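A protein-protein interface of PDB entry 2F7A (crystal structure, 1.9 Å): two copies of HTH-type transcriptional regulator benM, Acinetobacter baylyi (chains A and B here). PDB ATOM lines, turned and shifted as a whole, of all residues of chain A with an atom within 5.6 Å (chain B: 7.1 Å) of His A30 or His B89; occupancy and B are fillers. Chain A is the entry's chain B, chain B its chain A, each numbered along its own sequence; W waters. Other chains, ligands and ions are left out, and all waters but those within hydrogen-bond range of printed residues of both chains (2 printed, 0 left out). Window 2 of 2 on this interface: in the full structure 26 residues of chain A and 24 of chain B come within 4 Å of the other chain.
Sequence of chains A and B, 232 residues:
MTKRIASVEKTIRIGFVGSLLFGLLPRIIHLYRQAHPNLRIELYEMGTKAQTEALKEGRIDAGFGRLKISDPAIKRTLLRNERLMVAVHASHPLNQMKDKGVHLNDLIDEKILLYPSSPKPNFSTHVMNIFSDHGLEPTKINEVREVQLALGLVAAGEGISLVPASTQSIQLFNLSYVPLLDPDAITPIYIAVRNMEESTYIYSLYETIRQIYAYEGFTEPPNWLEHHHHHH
No position is printed for both chains.
Of the printed residues of chain B, Pro A26 touches Ala B155 and Ala B156. Printed residues of chain B within 4 Å of Arg A27: Phe B173 (3.0 Å). Ile A28 touches none of the printed residues of chain B. Of the printed residues of chain B, Ile A29 touches Ala B156. Of the printed residues of chain B, His A30 touches His B89 and Ala B156. His B89 touches just one residue of chain A: His A30 (3.4 Å). Of the printed residues of chain A, Ala B155 touches Pro A26 (3.6 Å). Gly B157 touches none of the printed residues of chain A. Of the printed residues of chain A, Glu B158 touches Arg A33. The nearest printed residue of chain A that does not touch His B89 is Pro A26 (6.1 Å). The nearest printed residue of chain A that does not touch Phe B173 is Pro A26 (5.6 Å).
Printed residues of chain B that touch a printed residue of chain A: His B89, Ala B155, Ala B156, Glu B158 and Phe B173. Hydrophobic or aromatic side chains of chain A that line the printed part of chain B: Pro A26, Ile A29 and His A30. Along chain A the printed residues that touch a printed residue of chain B span positions 26 to 33. Among the printed residues, 7 pairs touch across the chains.
A ring nitrogen (NE2) of His B89 sits at hydrogen-bond distance from a ring nitrogen (NE2) of His A30, at 3.4 Å. The side-chain carboxylate of Glu B158 lies within salt-bridge range of the guanidinium group of Arg A33 (3.1 Å).
The backbone carbonyl oxygen (O) of Ala B155 sits at hydrogen-bond distance from a ring nitrogen (ND1) of His B89 (2.9 Å). ND1 of His B89 sits close to O of Asn B174. O of Leu B153 is in hydrogen-bond range of N of Glu B158 (2.9 Å). O of His A30 lies within hydrogen-bond range of NE2 of Gln A34, 2.8 Å away.
CB of Pro A26 touches CB of Ala B155, at 3.6 Å. Ala B156 touches Pro A26. Arg A27 touches Phe B173. Ile A29 touches Ala B156. CD2 of His A30 touches O of Ala B156 (3.1 Å).
Water W2 lies within hydrogen-bond range of the side-chain carboxylate of Glu B158 and the guanidinium group of Arg A33. Water W1 bridges the side-chain hydroxyl of Ser B91 (3.2 Å) and a ring nitrogen (NE2) of His A30 (3.4 Å).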
ATOM      1  N   LEU A  25     -11.188  10.857  -7.969  1.00  0.00           N
ATOM      2  CA  LEU A  25     -11.995  11.550  -8.978  1.00  0.00           C
ATOM      3  C   LEU A  25     -12.127  10.787 -10.320  1.00  0.00           C
ATOM      4  O   LEU A  25     -13.244  10.616 -10.823  1.00  0.00           O
ATOM      5  CB  LEU A  25     -11.471  12.978  -9.192  1.00  0.00           C
ATOM      6  CG  LEU A  25     -12.235  13.888 -10.163  1.00  0.00           C
ATOM      7  CD1 LEU A  25     -13.721  13.940  -9.835  1.00  0.00           C
ATOM      8  CD2 LEU A  25     -11.625  15.284 -10.152  1.00  0.00           C
ATOM      9  N   PRO A  26     -11.003  10.328 -10.907  1.00  0.00           N
ATOM     10  CA  PRO A  26     -11.095   9.620 -12.187  1.00  0.00           C
ATOM     11  C   PRO A  26     -11.938   8.334 -12.173  1.00  0.00           C
ATOM     12  O   PRO A  26     -12.659   8.089 -13.130  1.00  0.00           O
ATOM     13  CB  PRO A  26      -9.628   9.306 -12.516  1.00  0.00           C
ATOM     14  CG  PRO A  26      -8.859  10.340 -11.780  1.00  0.00           C
ATOM     15  CD  PRO A  26      -9.600  10.461 -10.483  1.00  0.00           C
ATOM     16  N   ARG A  27     -11.848   7.524 -11.119  1.00  0.00           N
ATOM     17  CA  ARG A  27     -12.647   6.288 -11.041  1.00  0.00           C
ATOM     18  C   ARG A  27     -14.143   6.590 -10.871  1.00  0.00           C
ATOM     19  O   ARG A  27     -14.991   5.833 -11.353  1.00  0.00           O
ATOM     20  CB  ARG A  27     -12.140   5.334  -9.937  1.00  0.00           C
ATOM     21  CG  ARG A  27     -12.145   5.918  -8.526  1.00  0.00           C
ATOM     22  CD  ARG A  27     -12.250   4.873  -7.418  1.00  0.00           C
ATOM     23  NE  ARG A  27     -11.095   3.990  -7.219  1.00  0.00           N
ATOM     24  CZ  ARG A  27      -9.898   4.353  -6.745  1.00  0.00           C
ATOM     25  NH1 ARG A  27      -9.607   5.616  -6.469  1.00  0.00           N
ATOM     26  NH2 ARG A  27      -8.958   3.434  -6.573  1.00  0.00           N
ATOM     27  N   ILE A  28     -14.456   7.698 -10.198  1.00  0.00           N
ATOM     28  CA  ILE A  28     -15.832   8.174 -10.088  1.00  0.00           C
ATOM     29  C   ILE A  28     -16.354   8.566 -11.475  1.00  0.00           C
ATOM     30  O   ILE A  28     -17.385   8.077 -11.912  1.00  0.00           O
ATOM     31  CB  ILE A  28     -15.958   9.366  -9.097  1.00  0.00           C
ATOM     32  CG1 ILE A  28     -15.727   8.887  -7.661  1.00  0.00           C
ATOM     33  CG2 ILE A  28     -17.344  10.042  -9.220  1.00  0.00           C
ATOM     34  CD1 ILE A  28     -15.589  10.004  -6.644  1.00  0.00           C
ATOM     35  N   ILE A  29     -15.619   9.426 -12.171  1.00  0.00           N
ATOM     36  CA  ILE A  29     -15.982   9.830 -13.530  1.00  0.00           C
ATOM     37  C   ILE A  29     -16.123   8.637 -14.481  1.00  0.00           C
ATOM     38  O   ILE A  29     -17.009   8.631 -15.336  1.00  0.00           O
ATOM     39  CB  ILE A  29     -14.966  10.840 -14.105  1.00  0.00           C
ATOM     40  CG1 ILE A  29     -15.072  12.164 -13.354  1.00  0.00           C
ATOM     41  CG2 ILE A  29     -15.214  11.076 -15.601  1.00  0.00           C
ATOM     42  CD1 ILE A  29     -13.819  13.002 -13.435  1.00  0.00           C
ATOM     43  N   HIS A  30     -15.266   7.628 -14.328  1.00  0.00           N
ATOM     44  CA  HIS A  30     -15.317   6.452 -15.195  1.00  0.00           C
ATOM     45  C   HIS A  30     -16.586   5.628 -14.986  1.00  0.00           C
ATOM     46  O   HIS A  30     -17.232   5.236 -15.955  1.00  0.00           O
ATOM     47  CB  HIS A  30     -14.091   5.560 -15.004  1.00  0.00           C
ATOM     48  CG  HIS A  30     -14.113   4.331 -15.859  1.00  0.00           C
ATOM     49  ND1 HIS A  30     -14.636   3.133 -15.422  1.00  0.00           N
ATOM     50  CD2 HIS A  30     -13.719   4.125 -17.140  1.00  0.00           C
ATOM     51  CE1 HIS A  30     -14.540   2.234 -16.386  1.00  0.00           C
ATOM     52  NE2 HIS A  30     -13.986   2.811 -17.438  1.00  0.00           N
ATOM     53  N   LEU A  31     -16.937   5.364 -13.729  1.00  0.00           N
ATOM     54  CA  LEU A  31     -18.196   4.685 -13.401  1.00  0.00           C
ATOM     55  C   LEU A  31     -19.398   5.542 -13.818  1.00  0.00           C
ATOM     56  O   LEU A  31     -20.406   5.020 -14.314  1.00  0.00           O
ATOM     57  CB  LEU A  31     -18.257   4.379 -11.901  1.00  0.00           C
ATOM     58  CG  LEU A  31     -19.419   3.527 -11.366  1.00  0.00           C
ATOM     59  CD1 LEU A  31     -19.345   2.094 -11.881  1.00  0.00           C
ATOM     60  CD2 LEU A  31     -19.434   3.524  -9.840  1.00  0.00           C
ATOM     61  N   TYR A  32     -19.274   6.854 -13.620  1.00  0.00           N
ATOM     62  CA  TYR A  32     -20.294   7.824 -14.026  1.00  0.00           C
ATOM     63  C   TYR A  32     -20.545   7.765 -15.538  1.00  0.00           C
ATOM     64  O   TYR A  32     -21.697   7.768 -15.989  1.00  0.00           O
ATOM     65  CB  TYR A  32     -19.856   9.234 -13.602  1.00  0.00           C
ATOM     66  CG  TYR A  32     -20.883  10.322 -13.823  1.00  0.00           C
ATOM     67  CD1 TYR A  32     -22.062  10.357 -13.079  1.00  0.00           C
ATOM     68  CD2 TYR A  32     -20.667  11.332 -14.753  1.00  0.00           C
ATOM     69  CE1 TYR A  32     -23.006  11.356 -13.273  1.00  0.00           C
ATOM     70  CE2 TYR A  32     -21.605  12.336 -14.955  1.00  0.00           C
ATOM     71  CZ  TYR A  32     -22.772  12.343 -14.212  1.00  0.00           C
ATOM     72  OH  TYR A  32     -23.708  13.332 -14.409  1.00  0.00           O
ATOM     73  N   ARG A  33     -19.456   7.702 -16.307  1.00  0.00           N
ATOM     74  CA  ARG A  33     -19.513   7.570 -17.765  1.00  0.00           C
ATOM     75  C   ARG A  33     -20.299   6.332 -18.186  1.00  0.00           C
ATOM     76  O   ARG A  33     -21.114   6.399 -19.098  1.00  0.00           O
ATOM     77  CB  ARG A  33     -18.094   7.516 -18.353  1.00  0.00           C
ATOM     78  CG  ARG A  33     -17.991   7.033 -19.816  1.00  0.00           C
ATOM     79  CD  ARG A  33     -18.748   7.921 -20.791  1.00  0.00           C
ATOM     80  NE  ARG A  33     -18.155   9.252 -20.896  1.00  0.00           N
ATOM     81  CZ  ARG A  33     -18.758  10.308 -21.434  1.00  0.00           C
ATOM     82  NH1 ARG A  33     -19.996  10.212 -21.907  1.00  0.00           N
ATOM     83  NH2 ARG A  33     -18.125  11.475 -21.477  1.00  0.00           N
ATOM     84  N   GLN A  34     -20.056   5.206 -17.517  1.00  0.00           N
ATOM     85  CA  GLN A  34     -20.743   3.956 -17.859  1.00  0.00           C
ATOM     86  C   GLN A  34     -22.278   4.075 -17.777  1.00  0.00           C
ATOM     87  O   GLN A  34     -22.994   3.384 -18.513  1.00  0.00           O
ATOM     88  CB  GLN A  34     -20.247   2.792 -16.982  1.00  0.00           C
ATOM     89  CG  GLN A  34     -18.725   2.559 -16.983  1.00  0.00           C
ATOM     90  CD  GLN A  34     -18.056   2.818 -18.333  1.00  0.00           C
ATOM     91  OE1 GLN A  34     -18.375   2.172 -19.331  1.00  0.00           O
ATOM     92  NE2 GLN A  34     -17.113   3.761 -18.362  1.00  0.00           N
ATOM     93  N   VAL B  86       2.619   5.478 -23.717  1.00  0.00           N
ATOM     94  CA  VAL B  86       1.213   5.774 -23.885  1.00  0.00           C
ATOM     95  C   VAL B  86       0.488   5.457 -22.579  1.00  0.00           C
ATOM     96  O   VAL B  86       0.409   4.310 -22.173  1.00  0.00           O
ATOM     97  CB  VAL B  86       0.573   4.926 -25.014  1.00  0.00           C
ATOM     98  CG1 VAL B  86      -0.778   5.518 -25.418  1.00  0.00           C
ATOM     99  CG2 VAL B  86       1.488   4.831 -26.213  1.00  0.00           C
ATOM    100  N   ALA B  87      -0.038   6.484 -21.925  1.00  0.00           N
ATOM    101  CA  ALA B  87      -0.892   6.295 -20.770  1.00  0.00           C
ATOM    102  C   ALA B  87      -2.263   5.876 -21.274  1.00  0.00           C
ATOM    103  O   ALA B  87      -2.850   6.566 -22.095  1.00  0.00           O
ATOM    104  CB  ALA B  87      -0.990   7.585 -19.967  1.00  0.00           C
ATOM    105  N   VAL B  88      -2.756   4.737 -20.792  1.00  0.00           N
ATOM    106  CA  VAL B  88      -4.076   4.229 -21.165  1.00  0.00           C
ATOM    107  C   VAL B  88      -4.835   3.727 -19.936  1.00  0.00           C
ATOM    108  O   VAL B  88      -4.241   3.381 -18.916  1.00  0.00           O
ATOM    109  CB  VAL B  88      -3.978   3.075 -22.190  1.00  0.00           C
ATOM    110  CG1 VAL B  88      -3.120   3.479 -23.389  1.00  0.00           C
ATOM    111  CG2 VAL B  88      -3.433   1.809 -21.544  1.00  0.00           C
ATOM    112  N   HIS B  89      -6.153   3.681 -20.045  1.00  0.00           N
ATOM    113  CA  HIS B  89      -6.980   3.100 -19.005  1.00  0.00           C
ATOM    114  C   HIS B  89      -6.776   1.586 -18.977  1.00  0.00           C
ATOM    115  O   HIS B  89      -6.675   0.944 -20.027  1.00  0.00           O
ATOM    116  CB  HIS B  89      -8.451   3.435 -19.241  1.00  0.00           C
ATOM    117  CG  HIS B  89      -9.337   3.079 -18.092  1.00  0.00           C
ATOM    118  ND1 HIS B  89      -9.478   3.887 -16.988  1.00  0.00           N
ATOM    119  CD2 HIS B  89     -10.123   2.002 -17.871  1.00  0.00           C
ATOM    120  CE1 HIS B  89     -10.311   3.322 -16.134  1.00  0.00           C
ATOM    121  NE2 HIS B  89     -10.714   2.173 -16.644  1.00  0.00           N
ATOM    122  N   ALA B  90      -6.740   1.024 -17.772  1.00  0.00           N
ATOM    123  CA  ALA B  90      -6.399  -0.379 -17.566  1.00  0.00           C
ATOM    124  C   ALA B  90      -7.206  -1.317 -18.464  1.00  0.00           C
ATOM    125  O   ALA B  90      -6.690  -2.345 -18.907  1.00  0.00           O
ATOM    126  CB  ALA B  90      -6.595  -0.758 -16.104  1.00  0.00           C
ATOM    127  N   SER B  91      -8.457  -0.942 -18.731  1.00  0.00           N
ATOM    128  CA  SER B  91      -9.384  -1.738 -19.534  1.00  0.00           C
ATOM    129  C   SER B  91      -9.404  -1.371 -21.021  1.00  0.00           C
ATOM    130  O   SER B  91     -10.295  -1.805 -21.746  1.00  0.00           O
ATOM    131  CB  SER B  91     -10.804  -1.587 -18.974  1.00  0.00           C
ATOM    132  OG  SER B  91     -11.410  -0.395 -19.451  1.00  0.00           O
ATOM    133  N   HIS B  92      -8.442  -0.572 -21.471  1.00  0.00           N
ATOM    134  CA  HIS B  92      -8.325  -0.222 -22.889  1.00  0.00           C
ATOM    135  C   HIS B  92      -7.632  -1.379 -23.630  1.00  0.00           C
ATOM    136  O   HIS B  92      -6.698  -1.968 -23.092  1.00  0.00           O
ATOM    137  CB  HIS B  92      -7.512   1.078 -23.020  1.00  0.00           C
ATOM    138  CG  HIS B  92      -7.530   1.691 -24.389  1.00  0.00           C
ATOM    139  ND1 HIS B  92      -8.179   2.873 -24.670  1.00  0.00           N
ATOM    140  CD2 HIS B  92      -6.953   1.298 -25.546  1.00  0.00           C
ATOM    141  CE1 HIS B  92      -8.012   3.173 -25.945  1.00  0.00           C
ATOM    142  NE2 HIS B  92      -7.270   2.232 -26.500  1.00  0.00           N
ATOM    143  N   PRO B  93      -8.088  -1.721 -24.856  1.00  0.00           N
ATOM    144  CA  PRO B  93      -7.440  -2.801 -25.630  1.00  0.00           C
ATOM    145  C   PRO B  93      -5.914  -2.686 -25.799  1.00  0.00           C
ATOM    146  O   PRO B  93      -5.204  -3.676 -25.618  1.00  0.00           O
ATOM    147  CB  PRO B  93      -8.134  -2.729 -27.002  1.00  0.00           C
ATOM    148  CG  PRO B  93      -8.926  -1.463 -26.998  1.00  0.00           C
ATOM    149  CD  PRO B  93      -9.244  -1.163 -25.578  1.00  0.00           C
ATOM    150  N   LEU B  94      -5.427  -1.504 -26.170  1.00  0.00           N
ATOM    151  CA  LEU B  94      -3.974  -1.207 -26.192  1.00  0.00           C
ATOM    152  C   LEU B  94      -3.204  -1.649 -24.945  1.00  0.00           C
ATOM    153  O   LEU B  94      -2.007  -1.931 -25.032  1.00  0.00           O
ATOM    154  CB  LEU B  94      -3.706   0.288 -26.405  1.00  0.00           C
ATOM    155  CG  LEU B  94      -4.038   0.917 -27.758  1.00  0.00           C
ATOM    156  CD1 LEU B  94      -3.846   2.424 -27.679  1.00  0.00           C
ATOM    157  CD2 LEU B  94      -3.184   0.333 -28.872  1.00  0.00           C
ATOM    158  N   ASN B  95      -3.869  -1.700 -23.792  1.00  0.00           N
ATOM    159  CA  ASN B  95      -3.204  -2.149 -22.574  1.00  0.00           C
ATOM    160  C   ASN B  95      -2.809  -3.627 -22.577  1.00  0.00           C
ATOM    161  O   ASN B  95      -1.964  -4.042 -21.789  1.00  0.00           O
ATOM    162  CB  ASN B  95      -4.044  -1.848 -21.331  1.00  0.00           C
ATOM    163  CG  ASN B  95      -3.229  -1.948 -20.056  1.00  0.00           C
ATOM    164  OD1 ASN B  95      -2.040  -1.620 -20.050  1.00  0.00           O
ATOM    165  ND2 ASN B  95      -3.844  -2.428 -18.984  1.00  0.00           N
ATOM    166  N   LEU B 153      -7.869  12.219 -16.915  1.00  0.00           N
ATOM    167  CA  LEU B 153      -8.889  11.871 -17.906  1.00  0.00           C
ATOM    168  C   LEU B 153      -8.624  10.499 -18.522  1.00  0.00           C
ATOM    169  O   LEU B 153      -9.560   9.761 -18.827  1.00  0.00           O
ATOM    170  CB  LEU B 153      -8.971  12.944 -18.989  1.00  0.00           C
ATOM    171  CG  LEU B 153      -9.580  14.269 -18.512  1.00  0.00           C
ATOM    172  CD1 LEU B 153      -9.145  15.419 -19.410  1.00  0.00           C
ATOM    173  CD2 LEU B 153     -11.100  14.180 -18.445  1.00  0.00           C
ATOM    174  N   VAL B 154      -7.350  10.145 -18.687  1.00  0.00           N
ATOM    175  CA  VAL B 154      -6.995   8.788 -19.117  1.00  0.00           C
ATOM    176  C   VAL B 154      -7.405   7.772 -18.049  1.00  0.00           C
ATOM    177  O   VAL B 154      -7.977   6.731 -18.371  1.00  0.00           O
ATOM    178  CB  VAL B 154      -5.481   8.637 -19.409  1.00  0.00           C
ATOM    179  CG1 VAL B 154      -5.108   7.168 -19.582  1.00  0.00           C
ATOM    180  CG2 VAL B 154      -5.089   9.429 -20.640  1.00  0.00           C
ATOM    181  N   ALA B 155      -7.099   8.072 -16.786  1.00  0.00           N
ATOM    182  CA  ALA B 155      -7.512   7.220 -15.664  1.00  0.00           C
ATOM    183  C   ALA B 155      -9.032   7.124 -15.568  1.00  0.00           C
ATOM    184  O   ALA B 155      -9.570   6.117 -15.106  1.00  0.00           O
ATOM    185  CB  ALA B 155      -6.942   7.741 -14.368  1.00  0.00           C
ATOM    186  N   ALA B 156      -9.717   8.175 -16.010  1.00  0.00           N
ATOM    187  CA  ALA B 156     -11.172   8.158 -16.131  1.00  0.00           C
ATOM    188  C   ALA B 156     -11.657   7.379 -17.364  1.00  0.00           C
ATOM    189  O   ALA B 156     -12.853   7.113 -17.497  1.00  0.00           O
ATOM    190  CB  ALA B 156     -11.706   9.586 -16.164  1.00  0.00           C
ATOM    191  N   GLY B 157     -10.748   7.015 -18.264  1.00  0.00           N
ATOM    192  CA  GLY B 157     -11.101   6.209 -19.440  1.00  0.00           C
ATOM    193  C   GLY B 157     -11.662   7.022 -20.593  1.00  0.00           C
ATOM    194  O   GLY B 157     -12.359   6.486 -21.454  1.00  0.00           O
ATOM    195  N   GLU B 158     -11.337   8.311 -20.621  1.00  0.00           N
ATOM    196  CA  GLU B 158     -11.819   9.224 -21.658  1.00  0.00           C
ATOM    197  C   GLU B 158     -10.865   9.360 -22.862  1.00  0.00           C
ATOM    198  O   GLU B 158     -11.180  10.053 -23.830  1.00  0.00           O
ATOM    199  CB  GLU B 158     -12.093  10.599 -21.036  1.00  0.00           C
ATOM    200  CG  GLU B 158     -13.214  10.595 -19.995  1.00  0.00           C
ATOM    201  CD  GLU B 158     -14.570  10.268 -20.603  1.00  0.00           C
ATOM    202  OE1 GLU B 158     -15.077  11.091 -21.396  1.00  0.00           O
ATOM    203  OE2 GLU B 158     -15.119   9.188 -20.297  1.00  0.00           O
ATOM    204  N   GLY B 159      -9.713   8.695 -22.811  1.00  0.00           N
ATOM    205  CA  GLY B 159      -8.768   8.711 -23.928  1.00  0.00           C
ATOM    206  C   GLY B 159      -7.392   8.187 -23.548  1.00  0.00           C
ATOM    207  O   GLY B 159      -7.241   7.487 -22.544  1.00  0.00           O
ATOM    208  N   ILE B 160      -6.392   8.519 -24.362  1.00  0.00           N
ATOM    209  CA  ILE B 160      -5.003   8.145 -24.087  1.00  0.00           C
ATOM    210  C   ILE B 160      -4.112   9.377 -24.155  1.00  0.00           C
ATOM    211  O   ILE B 160      -4.523  10.418 -24.661  1.00  0.00           O
ATOM    212  CB  ILE B 160      -4.489   7.061 -25.075  1.00  0.00           C
ATOM    213  CG1 ILE B 160      -4.412   7.594 -26.513  1.00  0.00           C
ATOM    214  CG2 ILE B 160      -5.391   5.834 -25.031  1.00  0.00           C
ATOM    215  CD1 ILE B 160      -3.821   6.596 -27.498  1.00  0.00           C
ATOM    216  N   PHE B 173      -4.902   4.853  -9.967  1.00  0.00           N
ATOM    217  CA  PHE B 173      -5.720   3.658 -10.064  1.00  0.00           C
ATOM    218  C   PHE B 173      -6.282   3.509 -11.479  1.00  0.00           C
ATOM    219  O   PHE B 173      -6.782   4.478 -12.055  1.00  0.00           O
ATOM    220  CB  PHE B 173      -6.863   3.727  -9.057  1.00  0.00           C
ATOM    221  CG  PHE B 173      -7.814   2.584  -9.158  1.00  0.00           C
ATOM    222  CD1 PHE B 173      -7.461   1.333  -8.663  1.00  0.00           C
ATOM    223  CD2 PHE B 173      -9.062   2.748  -9.737  1.00  0.00           C
ATOM    224  CE1 PHE B 173      -8.335   0.265  -8.745  1.00  0.00           C
ATOM    225  CE2 PHE B 173      -9.940   1.689  -9.819  1.00  0.00           C
ATOM    226  CZ  PHE B 173      -9.576   0.439  -9.319  1.00  0.00           C
ATOM    227  N   ASN B 174      -6.179   2.292 -12.020  1.00  0.00           N
ATOM    228  CA  ASN B 174      -6.663   1.931 -13.368  1.00  0.00           C
ATOM    229  C   ASN B 174      -5.989   2.662 -14.538  1.00  0.00           C
ATOM    230  O   ASN B 174      -6.525   2.700 -15.653  1.00  0.00           O
ATOM    231  CB  ASN B 174      -8.191   2.063 -13.460  1.00  0.00           C
ATOM    232  CG  ASN B 174      -8.923   0.835 -12.943  1.00  0.00           C
ATOM    233  OD1 ASN B 174      -8.318  -0.099 -12.407  1.00  0.00           O
ATOM    234  ND2 ASN B 174     -10.235   0.831 -13.111  1.00  0.00           N
ATOM    235  N   LEU B 175      -4.800   3.198 -14.280  1.00  0.00           N
ATOM    236  CA  LEU B 175      -3.956   3.816 -15.295  1.00  0.00           C
ATOM    237  C   LEU B 175      -2.753   2.909 -15.556  1.00  0.00           C
ATOM    238  O   LEU B 175      -2.076   2.473 -14.624  1.00  0.00           O
ATOM    239  CB  LEU B 175      -3.483   5.190 -14.807  1.00  0.00           C
ATOM    240  CG  LEU B 175      -2.516   6.006 -15.674  1.00  0.00           C
ATOM    241  CD1 LEU B 175      -3.205   6.534 -16.886  1.00  0.00           C
ATOM    242  CD2 LEU B 175      -1.952   7.163 -14.852  1.00  0.00           C
ATOM    243  N   SER B 176      -2.493   2.629 -16.826  1.00  0.00           N
ATOM    244  CA  SER B 176      -1.364   1.796 -17.226  1.00  0.00           C
ATOM    245  C   SER B 176      -0.456   2.561 -18.181  1.00  0.00           C
ATOM    246  O   SER B 176      -0.934   3.338 -18.998  1.00  0.00           O
ATOM    247  CB  SER B 176      -1.890   0.544 -17.914  1.00  0.00           C
ATOM    248  OG  SER B 176      -0.843  -0.377 -18.123  1.00  0.00           O
HETATM  249  O   HOH W   1     -14.422  -0.473 -18.296  1.00  0.00           O
HETATM  250  O   HOH W   2     -15.931   8.263 -22.783  1.00  0.00           O
